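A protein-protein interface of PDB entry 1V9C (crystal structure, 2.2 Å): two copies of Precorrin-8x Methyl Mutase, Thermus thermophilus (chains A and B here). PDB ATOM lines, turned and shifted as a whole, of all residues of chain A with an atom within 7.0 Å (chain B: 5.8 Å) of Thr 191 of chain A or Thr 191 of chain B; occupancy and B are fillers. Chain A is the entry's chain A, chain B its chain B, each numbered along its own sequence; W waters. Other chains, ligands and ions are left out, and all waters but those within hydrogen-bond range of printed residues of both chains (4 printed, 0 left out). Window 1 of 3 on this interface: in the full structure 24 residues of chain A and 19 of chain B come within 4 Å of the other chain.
The backbone NH (N) of Val 161 of chain A sits at hydrogen-bond distance from the backbone carbonyl oxygen (O) of Gly 134 of chain A (3.4 Å).
The side-chain amide nitrogen (ND2) of Asn 135 of chain A is in hydrogen-bond range of the side-chain hydroxyl (OG) of Ser 190 of chain A (3.2 Å).
Printed residues of chain A that touch a printed residue of chain B: Met 75, Val 161, Ser 190, Thr 191 and Val 194.
Among the printed residues, no Asp or Glu carboxylate lies within 4 Å of a Lys or Arg side-chain nitrogen of the other chain.
Water W1 lies within hydrogen-bond range of OG1 of Thr 191 of chain A and N of Thr 191 of chain B.
Water W2 bridges O of Gly 188 of chain A (2.8 Å) and O of Ala 39 of chain B (2.9 Å).
Water W4 lies within hydrogen-bond range of OG1 of Thr 191 of chain B, N of Thr 191 of chain A and N of Ser 190 of chain A.
Water W3 lies within hydrogen-bond range of SD of Met 75 of chain B (3.1 Å) and OG1 of Thr 191 of chain A (3.1 Å).
Met 75 of chain B touches Met 75 of chain A (CE to CG, 3.2 Å).
CG2 of Val 161 of chain A touches O of Ala 39 of chain B (3.4 Å).
Thr 40 of chain B touches Val 161 of chain A (C to CG2, 3.5 Å).
Ser 190 of chain A touches Met 75 of chain B (CB to CE, 3.9 Å).
OG1 of Thr 191 of chain A touches OG1 of Thr 191 of chain B, at 3.6 Å.
Val 194 of chain A touches Met 75 of chain B (CG2 to CE, 3.6 Å).
Met 75 of chain B touches its own counterpart, Met 75 of chain A.
Ser 190 of chain A touches Met 75 of chain B, but with the chains exchanged Met 75 of chain A does not touch Ser 190 of chain B (4.9 Å).
Thr 191 of chain B touches its own counterpart, Thr 191 of chain A.
Val 194 of chain A touches Met 75 of chain B, but with the chains exchanged Met 75 of chain A does not touch Val 194 of chain B (4.4 Å).
12 positions are printed for both chains.
Thr 191 of chain A touches one residue of chain B.
Of the printed residues of chain B, Val 194 of chain A touches Met 75.
Ala 196 of chain A touches none of the printed residues of chain B.
Printed residues of chain A within 4 Å of Ala 39 of chain B: Val 161.
Printed residues of chain A within 4 Å of Thr 40 of chain B: Val 161.
Of the printed residues of chain A, Met 75 of chain B touches Met 75 (3.2 Å), Ser 190 (3.9 Å) and Val 194 (3.6 Å).
The nearest residue of chain B that does not touch Thr 191 of chain A is Met 75 of chain B (4.04 Å).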
ATOM      1  N   ARG A  35     -22.581  -8.346 -18.226  1.00  0.00           N
ATOM      2  CA  ARG A  35     -22.000  -7.865 -16.983  1.00  0.00           C
ATOM      3  C   ARG A  35     -20.942  -6.789 -17.230  1.00  0.00           C
ATOM      4  O   ARG A  35     -20.841  -5.828 -16.462  1.00  0.00           O
ATOM      5  CB  ARG A  35     -21.373  -9.039 -16.233  1.00  0.00           C
ATOM      6  CG  ARG A  35     -20.963  -8.702 -14.824  1.00  0.00           C
ATOM      7  CD  ARG A  35     -21.815  -9.473 -13.851  1.00  0.00           C
ATOM      8  NE  ARG A  35     -21.638  -9.018 -12.481  1.00  0.00           N
ATOM      9  CZ  ARG A  35     -22.267  -9.555 -11.443  1.00  0.00           C
ATOM     10  NH1 ARG A  35     -23.107 -10.564 -11.635  1.00  0.00           N
ATOM     11  NH2 ARG A  35     -22.055  -9.091 -10.219  1.00  0.00           N
ATOM     12  N   MET A  36     -20.160  -6.963 -18.300  1.00  0.00           N
ATOM     13  CA  MET A  36     -19.105  -6.025 -18.651  1.00  0.00           C
ATOM     14  C   MET A  36     -19.713  -4.720 -19.118  1.00  0.00           C
ATOM     15  O   MET A  36     -19.194  -3.648 -18.830  1.00  0.00           O
ATOM     16  CB  MET A  36     -18.211  -6.606 -19.754  1.00  0.00           C
ATOM     17  CG  MET A  36     -17.317  -7.770 -19.304  1.00  0.00           C
ATOM     18  SD  MET A  36     -16.508  -8.696 -20.670  1.00  0.00           S
ATOM     19  CE  MET A  36     -15.541  -7.398 -21.433  1.00  0.00           C
ATOM     20  N   ALA A  39     -21.197  -2.947 -16.120  1.00  0.00           N
ATOM     21  CA  ALA A  39     -20.201  -2.330 -15.258  1.00  0.00           C
ATOM     22  C   ALA A  39     -19.606  -1.052 -15.802  1.00  0.00           C
ATOM     23  O   ALA A  39     -19.024  -0.283 -15.046  1.00  0.00           O
ATOM     24  CB  ALA A  39     -19.077  -3.339 -14.951  1.00  0.00           C
ATOM     25  N   THR A  40     -19.762  -0.819 -17.103  1.00  0.00           N
ATOM     26  CA  THR A  40     -19.206   0.372 -17.733  1.00  0.00           C
ATOM     27  C   THR A  40     -20.210   1.324 -18.427  1.00  0.00           C
ATOM     28  O   THR A  40     -19.842   2.432 -18.797  1.00  0.00           O
ATOM     29  CB  THR A  40     -18.192  -0.035 -18.808  1.00  0.00           C
ATOM     30  OG1 THR A  40     -18.891  -0.732 -19.853  1.00  0.00           O
ATOM     31  CG2 THR A  40     -17.106  -0.977 -18.212  1.00  0.00           C
ATOM     32  N   MET A  75      -6.655  -3.390  -7.394  1.00  0.00           N
ATOM     33  CA  MET A  75      -8.026  -2.959  -7.642  1.00  0.00           C
ATOM     34  C   MET A  75      -8.863  -4.187  -8.017  1.00  0.00           C
ATOM     35  O   MET A  75     -10.024  -4.311  -7.630  1.00  0.00           O
ATOM     36  CB  MET A  75      -8.061  -1.931  -8.782  1.00  0.00           C
ATOM     37  CG  MET A  75      -9.443  -1.345  -9.038  1.00  0.00           C
ATOM     38  SD  MET A  75      -9.484   0.265  -9.933  1.00  0.00           S
ATOM     39  CE  MET A  75      -7.856   0.777  -9.844  1.00  0.00           C
ATOM     40  N   ILE A  76      -8.271  -5.103  -8.770  1.00  0.00           N
ATOM     41  CA  ILE A  76      -8.991  -6.315  -9.158  1.00  0.00           C
ATOM     42  C   ILE A  76      -9.246  -7.231  -7.958  1.00  0.00           C
ATOM     43  O   ILE A  76     -10.351  -7.731  -7.780  1.00  0.00           O
ATOM     44  CB  ILE A  76      -8.223  -7.099 -10.251  1.00  0.00           C
ATOM     45  CG1 ILE A  76      -8.143  -6.233 -11.520  1.00  0.00           C
ATOM     46  CG2 ILE A  76      -8.913  -8.458 -10.501  1.00  0.00           C
ATOM     47  CD1 ILE A  76      -7.480  -6.883 -12.675  1.00  0.00           C
ATOM     48  N   GLY A 134      -5.750  -6.524 -16.401  1.00  0.00           N
ATOM     49  CA  GLY A 134      -6.501  -5.335 -16.740  1.00  0.00           C
ATOM     50  C   GLY A 134      -5.632  -4.101 -16.825  1.00  0.00           C
ATOM     51  O   GLY A 134      -6.127  -3.025 -17.155  1.00  0.00           O
ATOM     52  N   ASN A 135      -4.335  -4.251 -16.568  1.00  0.00           N
ATOM     53  CA  ASN A 135      -3.429  -3.106 -16.579  1.00  0.00           C
ATOM     54  C   ASN A 135      -2.065  -3.248 -17.253  1.00  0.00           C
ATOM     55  O   ASN A 135      -1.721  -2.459 -18.124  1.00  0.00           O
ATOM     56  CB  ASN A 135      -3.212  -2.657 -15.141  1.00  0.00           C
ATOM     57  CG  ASN A 135      -4.508  -2.451 -14.413  1.00  0.00           C
ATOM     58  OD1 ASN A 135      -5.146  -1.404 -14.543  1.00  0.00           O
ATOM     59  ND2 ASN A 135      -4.933  -3.463 -13.662  1.00  0.00           N
ATOM     60  N   MET A 159      -7.457  -8.260 -20.814  1.00  0.00           N
ATOM     61  CA  MET A 159      -8.142  -6.980 -20.938  1.00  0.00           C
ATOM     62  C   MET A 159      -7.366  -5.751 -20.474  1.00  0.00           C
ATOM     63  O   MET A 159      -7.903  -4.910 -19.761  1.00  0.00           O
ATOM     64  CB  MET A 159      -9.464  -7.068 -20.189  1.00  0.00           C
ATOM     65  CG  MET A 159     -10.231  -8.328 -20.489  1.00  0.00           C
ATOM     66  SD  MET A 159     -11.758  -8.456 -19.526  1.00  0.00           S
ATOM     67  CE  MET A 159     -12.379  -9.993 -20.000  1.00  0.00           C
ATOM     68  N   VAL A 161      -5.968  -2.117 -20.399  1.00  0.00           N
ATOM     69  CA  VAL A 161      -6.473  -0.870 -20.977  1.00  0.00           C
ATOM     70  C   VAL A 161      -5.189  -0.110 -21.220  1.00  0.00           C
ATOM     71  O   VAL A 161      -4.247  -0.240 -20.441  1.00  0.00           O
ATOM     72  CB  VAL A 161      -7.396  -0.066 -19.974  1.00  0.00           C
ATOM     73  CG1 VAL A 161      -6.645   0.231 -18.690  1.00  0.00           C
ATOM     74  CG2 VAL A 161      -7.877   1.271 -20.610  1.00  0.00           C
ATOM     75  N   GLY A 188     -10.388  -1.669 -21.917  1.00  0.00           N
ATOM     76  CA  GLY A 188     -10.337  -2.749 -20.944  1.00  0.00           C
ATOM     77  C   GLY A 188     -10.135  -2.165 -19.553  1.00  0.00           C
ATOM     78  O   GLY A 188     -10.566  -1.039 -19.310  1.00  0.00           O
ATOM     79  N   GLY A 189      -9.487  -2.910 -18.651  1.00  0.00           N
ATOM     80  CA  GLY A 189      -9.243  -2.406 -17.303  1.00  0.00           C
ATOM     81  C   GLY A 189      -9.718  -3.277 -16.146  1.00  0.00           C
ATOM     82  O   GLY A 189     -10.451  -4.237 -16.344  1.00  0.00           O
ATOM     83  N   SER A 190      -9.312  -2.919 -14.928  1.00  0.00           N
ATOM     84  CA  SER A 190      -9.697  -3.671 -13.721  1.00  0.00           C
ATOM     85  C   SER A 190     -11.190  -3.924 -13.606  1.00  0.00           C
ATOM     86  O   SER A 190     -11.620  -5.014 -13.226  1.00  0.00           O
ATOM     87  CB  SER A 190      -9.239  -2.935 -12.470  1.00  0.00           C
ATOM     88  OG  SER A 190      -7.838  -2.776 -12.487  1.00  0.00           O
ATOM     89  N   THR A 191     -11.992  -2.921 -13.940  1.00  0.00           N
ATOM     90  CA  THR A 191     -13.435  -3.104 -13.860  1.00  0.00           C
ATOM     91  C   THR A 191     -13.963  -4.173 -14.824  1.00  0.00           C
ATOM     92  O   THR A 191     -14.912  -4.882 -14.510  1.00  0.00           O
ATOM     93  CB  THR A 191     -14.180  -1.783 -14.119  1.00  0.00           C
ATOM     94  OG1 THR A 191     -13.957  -0.890 -13.023  1.00  0.00           O
ATOM     95  CG2 THR A 191     -15.673  -2.032 -14.259  1.00  0.00           C
ATOM     96  N   LEU A 192     -13.359  -4.287 -15.999  1.00  0.00           N
ATOM     97  CA  LEU A 192     -13.816  -5.285 -16.954  1.00  0.00           C
ATOM     98  C   LEU A 192     -13.390  -6.665 -16.480  1.00  0.00           C
ATOM     99  O   LEU A 192     -14.144  -7.637 -16.595  1.00  0.00           O
ATOM    100  CB  LEU A 192     -13.240  -5.014 -18.348  1.00  0.00           C
ATOM    101  CG  LEU A 192     -13.958  -3.956 -19.196  1.00  0.00           C
ATOM    102  CD1 LEU A 192     -15.450  -4.229 -19.113  1.00  0.00           C
ATOM    103  CD2 LEU A 192     -13.636  -2.544 -18.735  1.00  0.00           C
ATOM    104  N   VAL A 193     -12.180  -6.752 -15.937  1.00  0.00           N
ATOM    105  CA  VAL A 193     -11.703  -8.029 -15.440  1.00  0.00           C
ATOM    106  C   VAL A 193     -12.611  -8.485 -14.308  1.00  0.00           C
ATOM    107  O   VAL A 193     -13.096  -9.617 -14.316  1.00  0.00           O
ATOM    108  CB  VAL A 193     -10.259  -7.945 -14.925  1.00  0.00           C
ATOM    109  CG1 VAL A 193      -9.861  -9.272 -14.331  1.00  0.00           C
ATOM    110  CG2 VAL A 193      -9.316  -7.578 -16.058  1.00  0.00           C
ATOM    111  N   VAL A 194     -12.873  -7.587 -13.358  1.00  0.00           N
ATOM    112  CA  VAL A 194     -13.725  -7.917 -12.212  1.00  0.00           C
ATOM    113  C   VAL A 194     -15.122  -8.322 -12.664  1.00  0.00           C
ATOM    114  O   VAL A 194     -15.684  -9.304 -12.176  1.00  0.00           O
ATOM    115  CB  VAL A 194     -13.860  -6.723 -11.213  1.00  0.00           C
ATOM    116  CG1 VAL A 194     -14.849  -7.083 -10.099  1.00  0.00           C
ATOM    117  CG2 VAL A 194     -12.501  -6.374 -10.615  1.00  0.00           C
ATOM    118  N   ALA A 195     -15.687  -7.546 -13.585  1.00  0.00           N
ATOM    119  CA  ALA A 195     -17.023  -7.826 -14.099  1.00  0.00           C
ATOM    120  C   ALA A 195     -17.096  -9.230 -14.728  1.00  0.00           C
ATOM    121  O   ALA A 195     -18.016  -9.995 -14.455  1.00  0.00           O
ATOM    122  CB  ALA A 195     -17.423  -6.752 -15.130  1.00  0.00           C
ATOM    123  N   ALA A 196     -16.110  -9.573 -15.554  1.00  0.00           N
ATOM    124  CA  ALA A 196     -16.104 -10.880 -16.200  1.00  0.00           C
ATOM    125  C   ALA A 196     -15.933 -12.019 -15.179  1.00  0.00           C
ATOM    126  O   ALA A 196     -16.484 -13.097 -15.360  1.00  0.00           O
ATOM    127  CB  ALA A 196     -14.993 -10.932 -17.288  1.00  0.00           C
ATOM    128  N   LEU A 197     -15.187 -11.772 -14.102  1.00  0.00           N
ATOM    129  CA  LEU A 197     -14.975 -12.786 -13.069  1.00  0.00           C
ATOM    130  C   LEU A 197     -16.244 -13.021 -12.273  1.00  0.00           C
ATOM    131  O   LEU A 197     -16.627 -14.164 -12.036  1.00  0.00           O
ATOM    132  CB  LEU A 197     -13.844 -12.377 -12.119  1.00  0.00           C
ATOM    133  CG  LEU A 197     -12.429 -12.436 -12.697  1.00  0.00           C
ATOM    134  CD1 LEU A 197     -11.429 -11.910 -11.663  1.00  0.00           C
ATOM    135  CD2 LEU A 197     -12.095 -13.870 -13.081  1.00  0.00           C
ATOM    136  N   ALA B  39      -7.086   6.410 -18.332  1.00  0.00           N
ATOM    137  CA  ALA B  39      -7.496   5.249 -17.537  1.00  0.00           C
ATOM    138  C   ALA B  39      -8.520   4.358 -18.215  1.00  0.00           C
ATOM    139  O   ALA B  39      -8.620   3.185 -17.915  1.00  0.00           O
ATOM    140  CB  ALA B  39      -8.040   5.715 -16.186  1.00  0.00           C
ATOM    141  N   THR B  40      -9.280   4.911 -19.147  1.00  0.00           N
ATOM    142  CA  THR B  40     -10.299   4.126 -19.819  1.00  0.00           C
ATOM    143  C   THR B  40     -10.101   3.932 -21.320  1.00  0.00           C
ATOM    144  O   THR B  40     -10.748   3.092 -21.917  1.00  0.00           O
ATOM    145  CB  THR B  40     -11.660   4.785 -19.642  1.00  0.00           C
ATOM    146  OG1 THR B  40     -11.623   6.080 -20.253  1.00  0.00           O
ATOM    147  CG2 THR B  40     -11.991   4.933 -18.154  1.00  0.00           C
ATOM    148  N   MET B  75     -12.792  -1.057  -4.506  1.00  0.00           N
ATOM    149  CA  MET B  75     -11.957  -0.934  -5.705  1.00  0.00           C
ATOM    150  C   MET B  75     -11.311   0.446  -5.733  1.00  0.00           C
ATOM    151  O   MET B  75     -10.147   0.592  -6.097  1.00  0.00           O
ATOM    152  CB  MET B  75     -12.781  -1.138  -6.989  1.00  0.00           C
ATOM    153  CG  MET B  75     -13.079  -2.589  -7.298  1.00  0.00           C
ATOM    154  SD  MET B  75     -13.677  -2.851  -8.988  1.00  0.00           S
ATOM    155  CE  MET B  75     -12.157  -2.878  -9.908  1.00  0.00           C
ATOM    156  N   ILE B  76     -12.081   1.461  -5.363  1.00  0.00           N
ATOM    157  CA  ILE B  76     -11.543   2.818  -5.312  1.00  0.00           C
ATOM    158  C   ILE B  76     -10.475   2.919  -4.221  1.00  0.00           C
ATOM    159  O   ILE B  76      -9.382   3.449  -4.452  1.00  0.00           O
ATOM    160  CB  ILE B  76     -12.666   3.844  -5.019  1.00  0.00           C
ATOM    161  CG1 ILE B  76     -13.608   3.902  -6.227  1.00  0.00           C
ATOM    162  CG2 ILE B  76     -12.084   5.203  -4.677  1.00  0.00           C
ATOM    163  CD1 ILE B  76     -14.762   4.859  -6.069  1.00  0.00           C
ATOM    164  N   GLY B 189     -17.683   5.150 -12.841  1.00  0.00           N
ATOM    165  CA  GLY B 189     -17.090   3.946 -12.273  1.00  0.00           C
ATOM    166  C   GLY B 189     -15.864   4.191 -11.416  1.00  0.00           C
ATOM    167  O   GLY B 189     -15.266   5.254 -11.475  1.00  0.00           O
ATOM    168  N   SER B 190     -15.494   3.188 -10.626  1.00  0.00           N
ATOM    169  CA  SER B 190     -14.331   3.255  -9.742  1.00  0.00           C
ATOM    170  C   SER B 190     -13.084   3.773 -10.430  1.00  0.00           C
ATOM    171  O   SER B 190     -12.370   4.634  -9.912  1.00  0.00           O
ATOM    172  CB  SER B 190     -14.039   1.866  -9.183  1.00  0.00           C
ATOM    173  OG  SER B 190     -15.122   1.388  -8.411  1.00  0.00           O
ATOM    174  N   THR B 191     -12.821   3.258 -11.624  1.00  0.00           N
ATOM    175  CA  THR B 191     -11.642   3.679 -12.355  1.00  0.00           C
ATOM    176  C   THR B 191     -11.626   5.184 -12.646  1.00  0.00           C
ATOM    177  O   THR B 191     -10.568   5.815 -12.661  1.00  0.00           O
ATOM    178  CB  THR B 191     -11.510   2.897 -13.674  1.00  0.00           C
ATOM    179  OG1 THR B 191     -11.343   1.502 -13.383  1.00  0.00           O
ATOM    180  CG2 THR B 191     -10.317   3.384 -14.440  1.00  0.00           C
ATOM    181  N   LEU B 192     -12.795   5.772 -12.859  1.00  0.00           N
ATOM    182  CA  LEU B 192     -12.819   7.195 -13.152  1.00  0.00           C
ATOM    183  C   LEU B 192     -12.531   7.988 -11.870  1.00  0.00           C
ATOM    184  O   LEU B 192     -11.773   8.939 -11.889  1.00  0.00           O
ATOM    185  CB  LEU B 192     -14.167   7.597 -13.784  1.00  0.00           C
ATOM    186  CG  LEU B 192     -14.498   7.190 -15.232  1.00  0.00           C
ATOM    187  CD1 LEU B 192     -13.478   7.822 -16.176  1.00  0.00           C
ATOM    188  CD2 LEU B 192     -14.524   5.664 -15.396  1.00  0.00           C
ATOM    189  N   VAL B 193     -13.114   7.583 -10.749  1.00  0.00           N
ATOM    190  CA  VAL B 193     -12.837   8.298  -9.501  1.00  0.00           C
ATOM    191  C   VAL B 193     -11.341   8.218  -9.175  1.00  0.00           C
ATOM    192  O   VAL B 193     -10.708   9.240  -8.909  1.00  0.00           O
ATOM    193  CB  VAL B 193     -13.606   7.708  -8.297  1.00  0.00           C
ATOM    194  CG1 VAL B 193     -13.381   8.578  -7.083  1.00  0.00           C
ATOM    195  CG2 VAL B 193     -15.079   7.659  -8.602  1.00  0.00           C
ATOM    196  N   VAL B 194     -10.780   7.005  -9.195  1.00  0.00           N
ATOM    197  CA  VAL B 194      -9.355   6.832  -8.898  1.00  0.00           C
ATOM    198  C   VAL B 194      -8.494   7.753  -9.795  1.00  0.00           C
ATOM    199  O   VAL B 194      -7.646   8.499  -9.310  1.00  0.00           O
ATOM    200  CB  VAL B 194      -8.925   5.345  -9.096  1.00  0.00           C
ATOM    201  CG1 VAL B 194      -7.410   5.212  -8.983  1.00  0.00           C
ATOM    202  CG2 VAL B 194      -9.623   4.445  -8.062  1.00  0.00           C
ATOM    203  N   ALA B 195      -8.735   7.714 -11.101  1.00  0.00           N
ATOM    204  CA  ALA B 195      -7.962   8.534 -12.046  1.00  0.00           C
ATOM    205  C   ALA B 195      -8.070  10.028 -11.750  1.00  0.00           C
ATOM    206  O   ALA B 195      -7.076  10.755 -11.815  1.00  0.00           O
ATOM    207  CB  ALA B 195      -8.411   8.240 -13.485  1.00  0.00           C
ATOM    208  N   ALA B 196      -9.282  10.479 -11.442  1.00  0.00           N
ATOM    209  CA  ALA B 196      -9.524  11.880 -11.112  1.00  0.00           C
ATOM    210  C   ALA B 196      -8.790  12.250  -9.805  1.00  0.00           C
ATOM    211  O   ALA B 196      -8.193  13.321  -9.701  1.00  0.00           O
ATOM    212  CB  ALA B 196     -11.040  12.135 -10.964  1.00  0.00           C
HETATM  213  O   HOH W   1     -14.579   1.766 -13.800  1.00  0.00           O
HETATM  214  O   HOH W   2     -10.330   0.942 -17.292  1.00  0.00           O
HETATM  215  O   HOH W   3     -15.884  -2.163 -10.979  1.00  0.00           O
HETATM  216  O   HOH W   4     -11.163  -0.497 -15.466  1.00  0.00           O
